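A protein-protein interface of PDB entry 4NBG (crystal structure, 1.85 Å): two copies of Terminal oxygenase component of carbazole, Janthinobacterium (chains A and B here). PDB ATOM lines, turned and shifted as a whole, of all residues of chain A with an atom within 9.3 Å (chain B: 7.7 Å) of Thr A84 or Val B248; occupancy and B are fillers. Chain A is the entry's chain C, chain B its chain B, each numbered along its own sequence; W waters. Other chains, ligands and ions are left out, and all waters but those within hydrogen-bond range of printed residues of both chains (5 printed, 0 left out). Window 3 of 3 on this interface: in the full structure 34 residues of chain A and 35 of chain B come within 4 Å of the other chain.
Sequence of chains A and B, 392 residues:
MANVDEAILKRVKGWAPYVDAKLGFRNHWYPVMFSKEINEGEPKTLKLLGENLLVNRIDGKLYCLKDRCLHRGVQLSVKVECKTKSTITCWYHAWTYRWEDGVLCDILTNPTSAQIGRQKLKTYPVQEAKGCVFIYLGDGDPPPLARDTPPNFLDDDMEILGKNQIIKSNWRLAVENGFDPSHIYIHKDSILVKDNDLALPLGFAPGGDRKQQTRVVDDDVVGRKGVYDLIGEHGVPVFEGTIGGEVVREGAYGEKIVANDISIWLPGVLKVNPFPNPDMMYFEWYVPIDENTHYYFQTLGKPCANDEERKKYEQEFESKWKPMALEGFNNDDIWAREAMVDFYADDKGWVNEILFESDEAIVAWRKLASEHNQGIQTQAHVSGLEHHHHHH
The side-chain carboxylate (OE1) of Glu A81 is in hydrogen-bond range of the side-chain hydroxyl (OH) of Tyr B185, 2.6 Å away. The backbone NH (N) of Gly B244 is in hydrogen-bond range of the side-chain carboxylate (OD2) of Asp A106 (2.9 Å).
Hydrophobic or aromatic side chains of chain B that line the printed part of chain A: Tyr B185, Ile B243 and Val B248. Along chain A the printed residues that touch a printed residue of chain B span positions 81 to 108. Among the printed residues, 15 pairs touch across the chains. Among the printed residues, no Asp or Glu carboxylate lies within 4 Å of a Lys or Arg side-chain nitrogen of the other chain.
Among the printed residues, merely in contact across the chains: Lys A83 with Tyr B185 (2.9 Å), Asp A106 with Ile B243 (3.3 Å), Lys A83 with Val B248 (3.5 Å), Thr A84 with Ile B243 (3.5 Å), Thr A89 with Ile B243 (3.7 Å), Lys A83 with Ile B243 (3.7 Å), Asp A106 with Thr B242 (3.7 Å), Leu A108 with Tyr B185 (3.8 Å), Ala A94 with Tyr B185 (3.9 Å), Thr A87 with Ile B243 (3.9 Å), Leu A108 with Thr B242 (3.9 Å), Thr A96 with Ile B243 (3.95 Å) and Thr A84 with Val B248 (3.98 Å).
No position is printed for both chains.
Water W2 lies within hydrogen-bond range of the side-chain carboxylate (OD2) of Asp A106 (2.7 Å) and the backbone NH (N) of Gly B244 (3.4 Å). Water W4 lies within hydrogen-bond range of O of Thr B242 (2.7 Å) and O of Ile A107 (3.3 Å). Water W3 lies within hydrogen-bond range of OG1 of Thr B242, OD1 of Asp A106, N of Gly B245 and N of Gly B244. Water W5 lies within hydrogen-bond range of NH1 of Arg B249 (2.8 Å) and NZ of Lys A83 (3.0 Å). Water W1 lies within hydrogen-bond range of the backbone carbonyl oxygen of Leu A108 (3.0 Å) and the backbone NH of Thr B242 (3.4 Å).
Printed residues of chain A within 4 Å of Val B248: Lys A83 (3.5 Å) and Thr A84 (3.98 Å). Of chain A, only Lys A83 (3.7 Å), Thr A84 (3.5 Å), Thr A87 (3.9 Å), Thr A89 (3.7 Å), Thr A96 (3.95 Å) and Asp A106 (3.3 Å) come within 4 Å of Ile B243. No residue of chain A comes within 4 Å of Val B247. Of the printed residues of chain B, Ala A94 touches Tyr B185 (3.9 Å). Of the printed residues of chain B, Leu A108 touches Tyr B185 (3.8 Å) and Thr B242 (3.9 Å). Glu B246 touches none of the printed residues of chain A. The nearest printed residue of chain A that does not touch Gly B244 is Cys A105 (5.7 Å).
The side-chain carboxylate (OE1) of Glu A81 is in salt-bridge range of the side-chain amino group (NZ) of Lys A83 (3.1 Å). The backbone carbonyl oxygen (O) of Glu A81 sits at hydrogen-bond distance from the backbone NH (N) of Thr A89, at 2.7 Å. The side-chain hydroxyl (OG1) of Thr A96 is in hydrogen-bond range of the side-chain hydroxyl (OG1) of Thr A89 (2.7 Å). The backbone carbonyl oxygen of Ala A94 sits at hydrogen-bond distance from the backbone NH of Leu A108, at 3.3 Å. The backbone NH (N) of Cys A105 is in hydrogen-bond range of the backbone carbonyl oxygen (O) of Thr A96 (3.0 Å). N of Thr A96 is in hydrogen-bond range of O of Asp A106, 2.7 Å away.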
ATOM      1  N   GLY A  41      18.607  -9.014  -7.993  1.00  0.00           N
ATOM      2  CA  GLY A  41      18.521  -9.569  -9.335  1.00  0.00           C
ATOM      3  C   GLY A  41      19.197  -8.758 -10.419  1.00  0.00           C
ATOM      4  O   GLY A  41      18.768  -8.769 -11.573  1.00  0.00           O
ATOM      5  N   PRO A  43      22.883  -8.706 -11.589  1.00  0.00           N
ATOM      6  CA  PRO A  43      24.267  -9.191 -11.610  1.00  0.00           C
ATOM      7  C   PRO A  43      25.286  -8.151 -12.064  1.00  0.00           C
ATOM      8  O   PRO A  43      25.084  -7.456 -13.060  1.00  0.00           O
ATOM      9  CB  PRO A  43      24.200 -10.380 -12.564  1.00  0.00           C
ATOM     10  CG  PRO A  43      22.814 -10.888 -12.368  1.00  0.00           C
ATOM     11  CD  PRO A  43      22.007  -9.614 -12.348  1.00  0.00           C
ATOM     12  N   ASN A  56      25.737 -11.093  -7.402  1.00  0.00           N
ATOM     13  CA  ASN A  56      24.305 -10.883  -7.531  1.00  0.00           C
ATOM     14  C   ASN A  56      23.671 -10.849  -6.148  1.00  0.00           C
ATOM     15  O   ASN A  56      24.203 -11.420  -5.195  1.00  0.00           O
ATOM     16  CB  ASN A  56      23.698 -12.008  -8.377  1.00  0.00           C
ATOM     17  CG  ASN A  56      22.251 -11.756  -8.746  1.00  0.00           C
ATOM     18  OD1 ASN A  56      21.791 -10.612  -8.791  1.00  0.00           O
ATOM     19  ND2 ASN A  56      21.529 -12.831  -9.040  1.00  0.00           N
ATOM     20  N   ILE A  58      20.290 -11.847  -4.158  1.00  0.00           N
ATOM     21  CA  ILE A  58      19.077 -12.657  -4.234  1.00  0.00           C
ATOM     22  C   ILE A  58      18.419 -12.707  -2.858  1.00  0.00           C
ATOM     23  O   ILE A  58      19.002 -13.212  -1.897  1.00  0.00           O
ATOM     24  CB  ILE A  58      19.396 -14.092  -4.695  1.00  0.00           C
ATOM     25  CG1 ILE A  58      20.175 -14.049  -6.014  1.00  0.00           C
ATOM     26  CG2 ILE A  58      18.102 -14.883  -4.869  1.00  0.00           C
ATOM     27  CD1 ILE A  58      20.618 -15.410  -6.514  1.00  0.00           C
ATOM     28  N   VAL A  80      23.731 -12.484 -19.849  1.00  0.00           N
ATOM     29  CA  VAL A  80      23.195 -13.077 -18.633  1.00  0.00           C
ATOM     30  C   VAL A  80      21.799 -13.662 -18.789  1.00  0.00           C
ATOM     31  O   VAL A  80      20.899 -13.022 -19.329  1.00  0.00           O
ATOM     32  CB  VAL A  80      23.165 -12.050 -17.484  1.00  0.00           C
ATOM     33  CG1 VAL A  80      22.587 -12.689 -16.229  1.00  0.00           C
ATOM     34  CG2 VAL A  80      24.571 -11.533 -17.218  1.00  0.00           C
ATOM     35  N   GLU A  81      21.634 -14.889 -18.306  1.00  0.00           N
ATOM     36  CA  GLU A  81      20.352 -15.573 -18.357  1.00  0.00           C
ATOM     37  C   GLU A  81      20.014 -16.190 -17.005  1.00  0.00           C
ATOM     38  O   GLU A  81      20.383 -17.329 -16.721  1.00  0.00           O
ATOM     39  CB  GLU A  81      20.357 -16.668 -19.435  1.00  0.00           C
ATOM     40  CG  GLU A  81      20.051 -16.166 -20.840  1.00  0.00           C
ATOM     41  CD  GLU A  81      19.929 -17.293 -21.859  1.00  0.00           C
ATOM     42  OE1 GLU A  81      19.410 -18.370 -21.498  1.00  0.00           O
ATOM     43  OE2 GLU A  81      20.335 -17.098 -23.022  1.00  0.00           O
ATOM     44  N   CYS A  82      19.332 -15.425 -16.159  1.00  0.00           N
ATOM     45  CA  CYS A  82      18.919 -15.937 -14.857  1.00  0.00           C
ATOM     46  C   CYS A  82      17.463 -16.356 -15.034  1.00  0.00           C
ATOM     47  O   CYS A  82      16.554 -15.533 -14.926  1.00  0.00           O
ATOM     48  CB  CYS A  82      19.049 -14.852 -13.786  1.00  0.00           C
ATOM     49  SG  CYS A  82      20.767 -14.380 -13.436  1.00  0.00           S
ATOM     50  N   LYS A  83      17.255 -17.638 -15.320  1.00  0.00           N
ATOM     51  CA  LYS A  83      15.918 -18.175 -15.563  1.00  0.00           C
ATOM     52  C   LYS A  83      15.124 -18.500 -14.309  1.00  0.00           C
ATOM     53  O   LYS A  83      13.892 -18.556 -14.340  1.00  0.00           O
ATOM     54  CB  LYS A  83      16.020 -19.399 -16.472  1.00  0.00           C
ATOM     55  CG  LYS A  83      16.676 -19.065 -17.800  1.00  0.00           C
ATOM     56  CD  LYS A  83      16.459 -20.147 -18.837  1.00  0.00           C
ATOM     57  CE  LYS A  83      17.013 -19.708 -20.172  1.00  0.00           C
ATOM     58  NZ  LYS A  83      16.471 -18.378 -20.577  1.00  0.00           N
ATOM     59  N   THR A  84      15.825 -18.738 -13.211  1.00  0.00           N
ATOM     60  CA  THR A  84      15.165 -18.993 -11.944  1.00  0.00           C
ATOM     61  C   THR A  84      15.881 -18.092 -10.956  1.00  0.00           C
ATOM     62  O   THR A  84      17.036 -17.714 -11.167  1.00  0.00           O
ATOM     63  CB  THR A  84      15.269 -20.463 -11.482  1.00  0.00           C
ATOM     64  OG1 THR A  84      16.616 -20.760 -11.104  1.00  0.00           O
ATOM     65  CG2 THR A  84      14.820 -21.401 -12.592  1.00  0.00           C
ATOM     66  N   LYS A  85      15.185 -17.743  -9.886  1.00  0.00           N
ATOM     67  CA  LYS A  85      15.724 -16.859  -8.867  1.00  0.00           C
ATOM     68  C   LYS A  85      17.070 -17.298  -8.292  1.00  0.00           C
ATOM     69  O   LYS A  85      17.937 -16.464  -8.028  1.00  0.00           O
ATOM     70  CB  LYS A  85      14.695 -16.732  -7.746  1.00  0.00           C
ATOM     71  CG  LYS A  85      14.872 -15.547  -6.833  1.00  0.00           C
ATOM     72  CD  LYS A  85      13.663 -15.454  -5.920  1.00  0.00           C
ATOM     73  CE  LYS A  85      13.745 -14.273  -4.985  1.00  0.00           C
ATOM     74  NZ  LYS A  85      12.545 -14.236  -4.107  1.00  0.00           N
ATOM     75  N   SER A  86      17.256 -18.603  -8.117  1.00  0.00           N
ATOM     76  CA  SER A  86      18.488 -19.117  -7.528  1.00  0.00           C
ATOM     77  C   SER A  86      19.539 -19.669  -8.489  1.00  0.00           C
ATOM     78  O   SER A  86      20.490 -20.317  -8.051  1.00  0.00           O
ATOM     79  CB  SER A  86      18.153 -20.203  -6.506  1.00  0.00           C
ATOM     80  OG  SER A  86      17.557 -21.318  -7.142  1.00  0.00           O
ATOM     81  N   THR A  87      19.387 -19.421  -9.783  1.00  0.00           N
ATOM     82  CA  THR A  87      20.362 -19.943 -10.738  1.00  0.00           C
ATOM     83  C   THR A  87      20.699 -18.982 -11.864  1.00  0.00           C
ATOM     84  O   THR A  87      20.040 -17.959 -12.059  1.00  0.00           O
ATOM     85  CB  THR A  87      19.867 -21.257 -11.405  1.00  0.00           C
ATOM     86  OG1 THR A  87      18.755 -20.972 -12.259  1.00  0.00           O
ATOM     87  CG2 THR A  87      19.447 -22.278 -10.363  1.00  0.00           C
ATOM     88  N   ILE A  88      21.752 -19.322 -12.599  1.00  0.00           N
ATOM     89  CA  ILE A  88      22.168 -18.548 -13.756  1.00  0.00           C
ATOM     90  C   ILE A  88      22.476 -19.580 -14.831  1.00  0.00           C
ATOM     91  O   ILE A  88      23.098 -20.610 -14.557  1.00  0.00           O
ATOM     92  CB  ILE A  88      23.422 -17.678 -13.480  1.00  0.00           C
ATOM     93  CG1 ILE A  88      23.799 -16.921 -14.756  1.00  0.00           C
ATOM     94  CG2 ILE A  88      24.579 -18.541 -12.987  1.00  0.00           C
ATOM     95  CD1 ILE A  88      24.910 -15.895 -14.582  1.00  0.00           C
ATOM     96  N   THR A  89      22.022 -19.309 -16.046  1.00  0.00           N
ATOM     97  CA  THR A  89      22.224 -20.227 -17.163  1.00  0.00           C
ATOM     98  C   THR A  89      23.149 -19.637 -18.215  1.00  0.00           C
ATOM     99  O   THR A  89      22.884 -18.557 -18.737  1.00  0.00           O
ATOM    100  CB  THR A  89      20.873 -20.564 -17.831  1.00  0.00           C
ATOM    101  OG1 THR A  89      20.034 -21.241 -16.886  1.00  0.00           O
ATOM    102  CG2 THR A  89      21.077 -21.447 -19.064  1.00  0.00           C
ATOM    103  N   ALA A  94      23.650 -23.511 -22.302  1.00  0.00           N
ATOM    104  CA  ALA A  94      22.722 -23.592 -21.180  1.00  0.00           C
ATOM    105  C   ALA A  94      23.119 -24.356 -19.919  1.00  0.00           C
ATOM    106  O   ALA A  94      22.242 -24.855 -19.203  1.00  0.00           O
ATOM    107  CB  ALA A  94      21.375 -24.108 -21.686  1.00  0.00           C
ATOM    108  N   THR A  96      23.602 -24.732 -16.348  1.00  0.00           N
ATOM    109  CA  THR A  96      23.009 -23.918 -15.295  1.00  0.00           C
ATOM    110  C   THR A  96      23.615 -24.151 -13.919  1.00  0.00           C
ATOM    111  O   THR A  96      23.775 -25.290 -13.480  1.00  0.00           O
ATOM    112  CB  THR A  96      21.489 -24.159 -15.261  1.00  0.00           C
ATOM    113  OG1 THR A  96      20.937 -23.794 -16.534  1.00  0.00           O
ATOM    114  CG2 THR A  96      20.827 -23.331 -14.173  1.00  0.00           C
ATOM    115  N   TYR A  97      23.946 -23.055 -13.241  1.00  0.00           N
ATOM    116  CA  TYR A  97      24.570 -23.121 -11.926  1.00  0.00           C
ATOM    117  C   TYR A  97      23.748 -22.426 -10.849  1.00  0.00           C
ATOM    118  O   TYR A  97      23.067 -21.437 -11.119  1.00  0.00           O
ATOM    119  CB  TYR A  97      25.951 -22.457 -11.958  1.00  0.00           C
ATOM    120  CG  TYR A  97      26.843 -22.880 -13.105  1.00  0.00           C
ATOM    121  CD1 TYR A  97      26.755 -22.262 -14.354  1.00  0.00           C
ATOM    122  CD2 TYR A  97      27.789 -23.887 -12.934  1.00  0.00           C
ATOM    123  CE1 TYR A  97      27.597 -22.641 -15.405  1.00  0.00           C
ATOM    124  CE2 TYR A  97      28.631 -24.272 -13.973  1.00  0.00           C
ATOM    125  CZ  TYR A  97      28.532 -23.647 -15.199  1.00  0.00           C
ATOM    126  OH  TYR A  97      29.384 -24.033 -16.212  1.00  0.00           O
ATOM    127  N   ARG A  98      23.825 -22.946  -9.628  1.00  0.00           N
ATOM    128  CA  ARG A  98      23.124 -22.346  -8.493  1.00  0.00           C
ATOM    129  C   ARG A  98      24.056 -21.291  -7.897  1.00  0.00           C
ATOM    130  O   ARG A  98      25.238 -21.554  -7.705  1.00  0.00           O
ATOM    131  CB  ARG A  98      22.811 -23.397  -7.421  1.00  0.00           C
ATOM    132  CG  ARG A  98      21.880 -24.513  -7.879  1.00  0.00           C
ATOM    133  CD  ARG A  98      21.378 -25.352  -6.709  1.00  0.00           C
ATOM    134  NE  ARG A  98      22.440 -26.076  -6.014  1.00  0.00           N
ATOM    135  CZ  ARG A  98      22.533 -27.402  -5.962  1.00  0.00           C
ATOM    136  NH1 ARG A  98      21.628 -28.158  -6.569  1.00  0.00           N
ATOM    137  NH2 ARG A  98      23.521 -27.979  -5.289  1.00  0.00           N
ATOM    138  N   TRP A  99      23.531 -20.105  -7.605  1.00  0.00           N
ATOM    139  CA  TRP A  99      24.357 -19.049  -7.025  1.00  0.00           C
ATOM    140  C   TRP A  99      24.855 -19.438  -5.639  1.00  0.00           C
ATOM    141  O   TRP A  99      25.952 -19.064  -5.232  1.00  0.00           O
ATOM    142  CB  TRP A  99      23.568 -17.740  -6.913  1.00  0.00           C
ATOM    143  CG  TRP A  99      23.319 -17.047  -8.212  1.00  0.00           C
ATOM    144  CD1 TRP A  99      22.213 -17.154  -9.005  1.00  0.00           C
ATOM    145  CD2 TRP A  99      24.190 -16.109  -8.862  1.00  0.00           C
ATOM    146  NE1 TRP A  99      22.335 -16.337 -10.105  1.00  0.00           N
ATOM    147  CE2 TRP A  99      23.540 -15.685 -10.042  1.00  0.00           C
ATOM    148  CE3 TRP A  99      25.456 -15.586  -8.560  1.00  0.00           C
ATOM    149  CZ2 TRP A  99      24.112 -14.760 -10.922  1.00  0.00           C
ATOM    150  CZ3 TRP A  99      26.026 -14.666  -9.437  1.00  0.00           C
ATOM    151  CH2 TRP A  99      25.353 -14.263 -10.603  1.00  0.00           C
ATOM    152  N   CYS A 105      23.587 -27.633 -11.694  1.00  0.00           N
ATOM    153  CA  CYS A 105      22.350 -28.348 -11.382  1.00  0.00           C
ATOM    154  C   CYS A 105      21.482 -28.778 -12.559  1.00  0.00           C
ATOM    155  O   CYS A 105      20.634 -29.661 -12.408  1.00  0.00           O
ATOM    156  CB  CYS A 105      21.504 -27.499 -10.433  1.00  0.00           C
ATOM    157  SG  CYS A 105      20.930 -25.957 -11.168  1.00  0.00           S
ATOM    158  N   ASP A 106      21.673 -28.145 -13.713  1.00  0.00           N
ATOM    159  CA  ASP A 106      20.900 -28.463 -14.915  1.00  0.00           C
ATOM    160  C   ASP A 106      21.648 -28.034 -16.179  1.00  0.00           C
ATOM    161  O   ASP A 106      22.546 -27.193 -16.131  1.00  0.00           O
ATOM    162  CB  ASP A 106      19.551 -27.730 -14.905  1.00  0.00           C
ATOM    163  CG  ASP A 106      18.527 -28.372 -13.981  1.00  0.00           C
ATOM    164  OD1 ASP A 106      18.069 -29.498 -14.278  1.00  0.00           O
ATOM    165  OD2 ASP A 106      18.174 -27.741 -12.961  1.00  0.00           O
ATOM    166  N   ILE A 107      21.264 -28.625 -17.305  1.00  0.00           N
ATOM    167  CA  ILE A 107      21.837 -28.283 -18.604  1.00  0.00           C
ATOM    168  C   ILE A 107      20.680 -28.383 -19.588  1.00  0.00           C
ATOM    169  O   ILE A 107      20.271 -29.478 -19.970  1.00  0.00           O
ATOM    170  CB  ILE A 107      22.959 -29.256 -19.035  1.00  0.00           C
ATOM    171  CG1 ILE A 107      24.123 -29.196 -18.039  1.00  0.00           C
ATOM    172  CG2 ILE A 107      23.445 -28.883 -20.434  1.00  0.00           C
ATOM    173  CD1 ILE A 107      25.305 -30.086 -18.409  1.00  0.00           C
ATOM    174  N   LEU A 108      20.148 -27.233 -19.986  1.00  0.00           N
ATOM    175  CA  LEU A 108      19.008 -27.191 -20.889  1.00  0.00           C
ATOM    176  C   LEU A 108      19.208 -27.864 -22.240  1.00  0.00           C
ATOM    177  O   LEU A 108      18.261 -28.418 -22.798  1.00  0.00           O
ATOM    178  CB  LEU A 108      18.555 -25.744 -21.101  1.00  0.00           C
ATOM    179  CG  LEU A 108      17.813 -25.079 -19.935  1.00  0.00           C
ATOM    180  CD1 LEU A 108      18.663 -25.107 -18.691  1.00  0.00           C
ATOM    181  CD2 LEU A 108      17.455 -23.651 -20.305  1.00  0.00           C
ATOM    182  N   TYR B 185      21.445 -23.450 -29.118  1.00  0.00           N
ATOM    183  CA  TYR B 185      20.764 -22.716 -28.054  1.00  0.00           C
ATOM    184  C   TYR B 185      20.887 -21.199 -28.220  1.00  0.00           C
ATOM    185  O   TYR B 185      19.971 -20.451 -27.867  1.00  0.00           O
ATOM    186  CB  TYR B 185      21.341 -23.128 -26.698  1.00  0.00           C
ATOM    187  CG  TYR B 185      20.649 -22.494 -25.516  1.00  0.00           C
ATOM    188  CD1 TYR B 185      19.387 -22.923 -25.112  1.00  0.00           C
ATOM    189  CD2 TYR B 185      21.246 -21.447 -24.812  1.00  0.00           C
ATOM    190  CE1 TYR B 185      18.733 -22.330 -24.038  1.00  0.00           C
ATOM    191  CE2 TYR B 185      20.600 -20.844 -23.735  1.00  0.00           C
ATOM    192  CZ  TYR B 185      19.342 -21.292 -23.354  1.00  0.00           C
ATOM    193  OH  TYR B 185      18.689 -20.700 -22.299  1.00  0.00           O
ATOM    194  N   LEU B 202      16.202 -26.800 -28.629  1.00  0.00           N
ATOM    195  CA  LEU B 202      17.139 -26.069 -27.783  1.00  0.00           C
ATOM    196  C   LEU B 202      18.428 -26.869 -27.664  1.00  0.00           C
ATOM    197  O   LEU B 202      19.489 -26.327 -27.364  1.00  0.00           O
ATOM    198  CB  LEU B 202      16.541 -25.862 -26.391  1.00  0.00           C
ATOM    199  CG  LEU B 202      15.260 -25.033 -26.290  1.00  0.00           C
ATOM    200  CD1 LEU B 202      14.761 -25.054 -24.850  1.00  0.00           C
ATOM    201  CD2 LEU B 202      15.526 -23.606 -26.746  1.00  0.00           C
ATOM    202  N   GLU B 240      11.696 -28.459 -24.520  1.00  0.00           N
ATOM    203  CA  GLU B 240      11.284 -27.890 -23.242  1.00  0.00           C
ATOM    204  C   GLU B 240      12.457 -27.920 -22.273  1.00  0.00           C
ATOM    205  O   GLU B 240      12.773 -28.965 -21.703  1.00  0.00           O
ATOM    206  CB  GLU B 240      10.101 -28.665 -22.651  1.00  0.00           C
ATOM    207  CG  GLU B 240       8.791 -28.465 -23.403  1.00  0.00           C
ATOM    208  CD  GLU B 240       7.593 -29.039 -22.663  1.00  0.00           C
ATOM    209  OE1 GLU B 240       7.360 -28.638 -21.501  1.00  0.00           O
ATOM    210  OE2 GLU B 240       6.879 -29.884 -23.244  1.00  0.00           O
ATOM    211  N   GLY B 241      13.107 -26.773 -22.107  1.00  0.00           N
ATOM    212  CA  GLY B 241      14.236 -26.685 -21.200  1.00  0.00           C
ATOM    213  C   GLY B 241      13.756 -26.499 -19.776  1.00  0.00           C
ATOM    214  O   GLY B 241      12.915 -25.638 -19.506  1.00  0.00           O
ATOM    215  N   THR B 242      14.295 -27.291 -18.856  1.00  0.00           N
ATOM    216  CA  THR B 242      13.881 -27.212 -17.463  1.00  0.00           C
ATOM    217  C   THR B 242      15.000 -26.993 -16.453  1.00  0.00           C
ATOM    218  O   THR B 242      16.155 -27.367 -16.674  1.00  0.00           O
ATOM    219  CB  THR B 242      13.149 -28.492 -17.037  1.00  0.00           C
ATOM    220  OG1 THR B 242      14.070 -29.590 -17.058  1.00  0.00           O
ATOM    221  CG2 THR B 242      11.990 -28.786 -17.975  1.00  0.00           C
ATOM    222  N   ILE B 243      14.625 -26.384 -15.334  1.00  0.00           N
ATOM    223  CA  ILE B 243      15.529 -26.130 -14.225  1.00  0.00           C
ATOM    224  C   ILE B 243      14.765 -26.580 -12.984  1.00  0.00           C
ATOM    225  O   ILE B 243      13.685 -26.068 -12.696  1.00  0.00           O
ATOM    226  CB  ILE B 243      15.875 -24.633 -14.089  1.00  0.00           C
ATOM    227  CG1 ILE B 243      16.683 -24.174 -15.306  1.00  0.00           C
ATOM    228  CG2 ILE B 243      16.657 -24.401 -12.805  1.00  0.00           C
ATOM    229  CD1 ILE B 243      17.081 -22.711 -15.270  1.00  0.00           C
ATOM    230  N   GLY B 244      15.316 -27.549 -12.263  1.00  0.00           N
ATOM    231  CA  GLY B 244      14.638 -28.037 -11.077  1.00  0.00           C
ATOM    232  C   GLY B 244      13.312 -28.689 -11.430  1.00  0.00           C
ATOM    233  O   GLY B 244      12.431 -28.824 -10.579  1.00  0.00           O
ATOM    234  N   GLY B 245      13.165 -29.084 -12.693  1.00  0.00           N
ATOM    235  CA  GLY B 245      11.943 -29.736 -13.131  1.00  0.00           C
ATOM    236  C   GLY B 245      10.927 -28.833 -13.802  1.00  0.00           C
ATOM    237  O   GLY B 245      10.051 -29.312 -14.524  1.00  0.00           O
ATOM    238  N   GLU B 246      11.031 -27.530 -13.568  1.00  0.00           N
ATOM    239  CA  GLU B 246      10.101 -26.579 -14.163  1.00  0.00           C
ATOM    240  C   GLU B 246      10.588 -26.037 -15.500  1.00  0.00           C
ATOM    241  O   GLU B 246      11.746 -25.646 -15.641  1.00  0.00           O
ATOM    242  CB  GLU B 246       9.837 -25.418 -13.199  1.00  0.00           C
ATOM    243  CG  GLU B 246       8.754 -25.713 -12.164  1.00  0.00           C
ATOM    244  CD  GLU B 246       9.035 -26.966 -11.356  1.00  0.00           C
ATOM    245  OE1 GLU B 246      10.004 -26.964 -10.567  1.00  0.00           O
ATOM    246  OE2 GLU B 246       8.288 -27.956 -11.515  1.00  0.00           O
ATOM    247  N   VAL B 247       9.693 -26.026 -16.482  1.00  0.00           N
ATOM    248  CA  VAL B 247      10.018 -25.528 -17.810  1.00  0.00           C
ATOM    249  C   VAL B 247      10.278 -24.030 -17.742  1.00  0.00           C
ATOM    250  O   VAL B 247       9.430 -23.264 -17.285  1.00  0.00           O
ATOM    251  CB  VAL B 247       8.862 -25.802 -18.800  1.00  0.00           C
ATOM    252  CG1 VAL B 247       9.201 -25.242 -20.174  1.00  0.00           C
ATOM    253  CG2 VAL B 247       8.605 -27.297 -18.889  1.00  0.00           C
ATOM    254  N   VAL B 248      11.458 -23.615 -18.189  1.00  0.00           N
ATOM    255  CA  VAL B 248      11.816 -22.205 -18.170  1.00  0.00           C
ATOM    256  C   VAL B 248      12.049 -21.671 -19.576  1.00  0.00           C
ATOM    257  O   VAL B 248      12.174 -20.464 -19.776  1.00  0.00           O
ATOM    258  CB  VAL B 248      13.083 -21.964 -17.322  1.00  0.00           C
ATOM    259  CG1 VAL B 248      12.835 -22.414 -15.893  1.00  0.00           C
ATOM    260  CG2 VAL B 248      14.264 -22.718 -17.918  1.00  0.00           C
ATOM    261  N   ARG B 249      12.099 -22.577 -20.549  1.00  0.00           N
ATOM    262  CA  ARG B 249      12.318 -22.191 -21.938  1.00  0.00           C
ATOM    263  C   ARG B 249      11.848 -23.268 -22.911  1.00  0.00           C
ATOM    264  O   ARG B 249      12.010 -24.458 -22.656  1.00  0.00           O
ATOM    265  CB  ARG B 249      13.804 -21.918 -22.189  1.00  0.00           C
ATOM    266  CG  ARG B 249      14.126 -21.625 -23.649  1.00  0.00           C
ATOM    267  CD  ARG B 249      13.743 -20.210 -24.034  1.00  0.00           C
ATOM    268  NE  ARG B 249      13.522 -20.067 -25.472  1.00  0.00           N
ATOM    269  CZ  ARG B 249      13.609 -18.915 -26.130  1.00  0.00           C
ATOM    270  NH1 ARG B 249      13.925 -17.801 -25.482  1.00  0.00           N
ATOM    271  NH2 ARG B 249      13.362 -18.870 -27.430  1.00  0.00           N
ATOM    272  N   GLU B 250      11.272 -22.841 -24.030  1.00  0.00           N
ATOM    273  CA  GLU B 250      10.800 -23.777 -25.043  1.00  0.00           C
ATOM    274  C   GLU B 250      11.491 -23.553 -26.380  1.00  0.00           C
ATOM    275  O   GLU B 250      11.904 -22.436 -26.700  1.00  0.00           O
ATOM    276  CB  GLU B 250       9.289 -23.645 -25.241  1.00  0.00           C
ATOM    277  CG  GLU B 250       8.455 -24.140 -24.078  1.00  0.00           C
ATOM    278  CD  GLU B 250       6.974 -24.136 -24.397  1.00  0.00           C
ATOM    279  OE1 GLU B 250       6.428 -23.046 -24.674  1.00  0.00           O
ATOM    280  OE2 GLU B 250       6.358 -25.225 -24.375  1.00  0.00           O
HETATM  281  O   HOH W   1      16.259 -29.322 -20.785  1.00  0.00           O
HETATM  282  O   HOH W   2      17.965 -28.471 -10.406  1.00  0.00           O
HETATM  283  O   HOH W   3      15.290 -30.012 -14.595  1.00  0.00           O
HETATM  284  O   HOH W   4      17.395 -29.028 -18.423  1.00  0.00           O
HETATM  285  O   HOH W   5      14.956 -17.147 -22.909  1.00  0.00           O
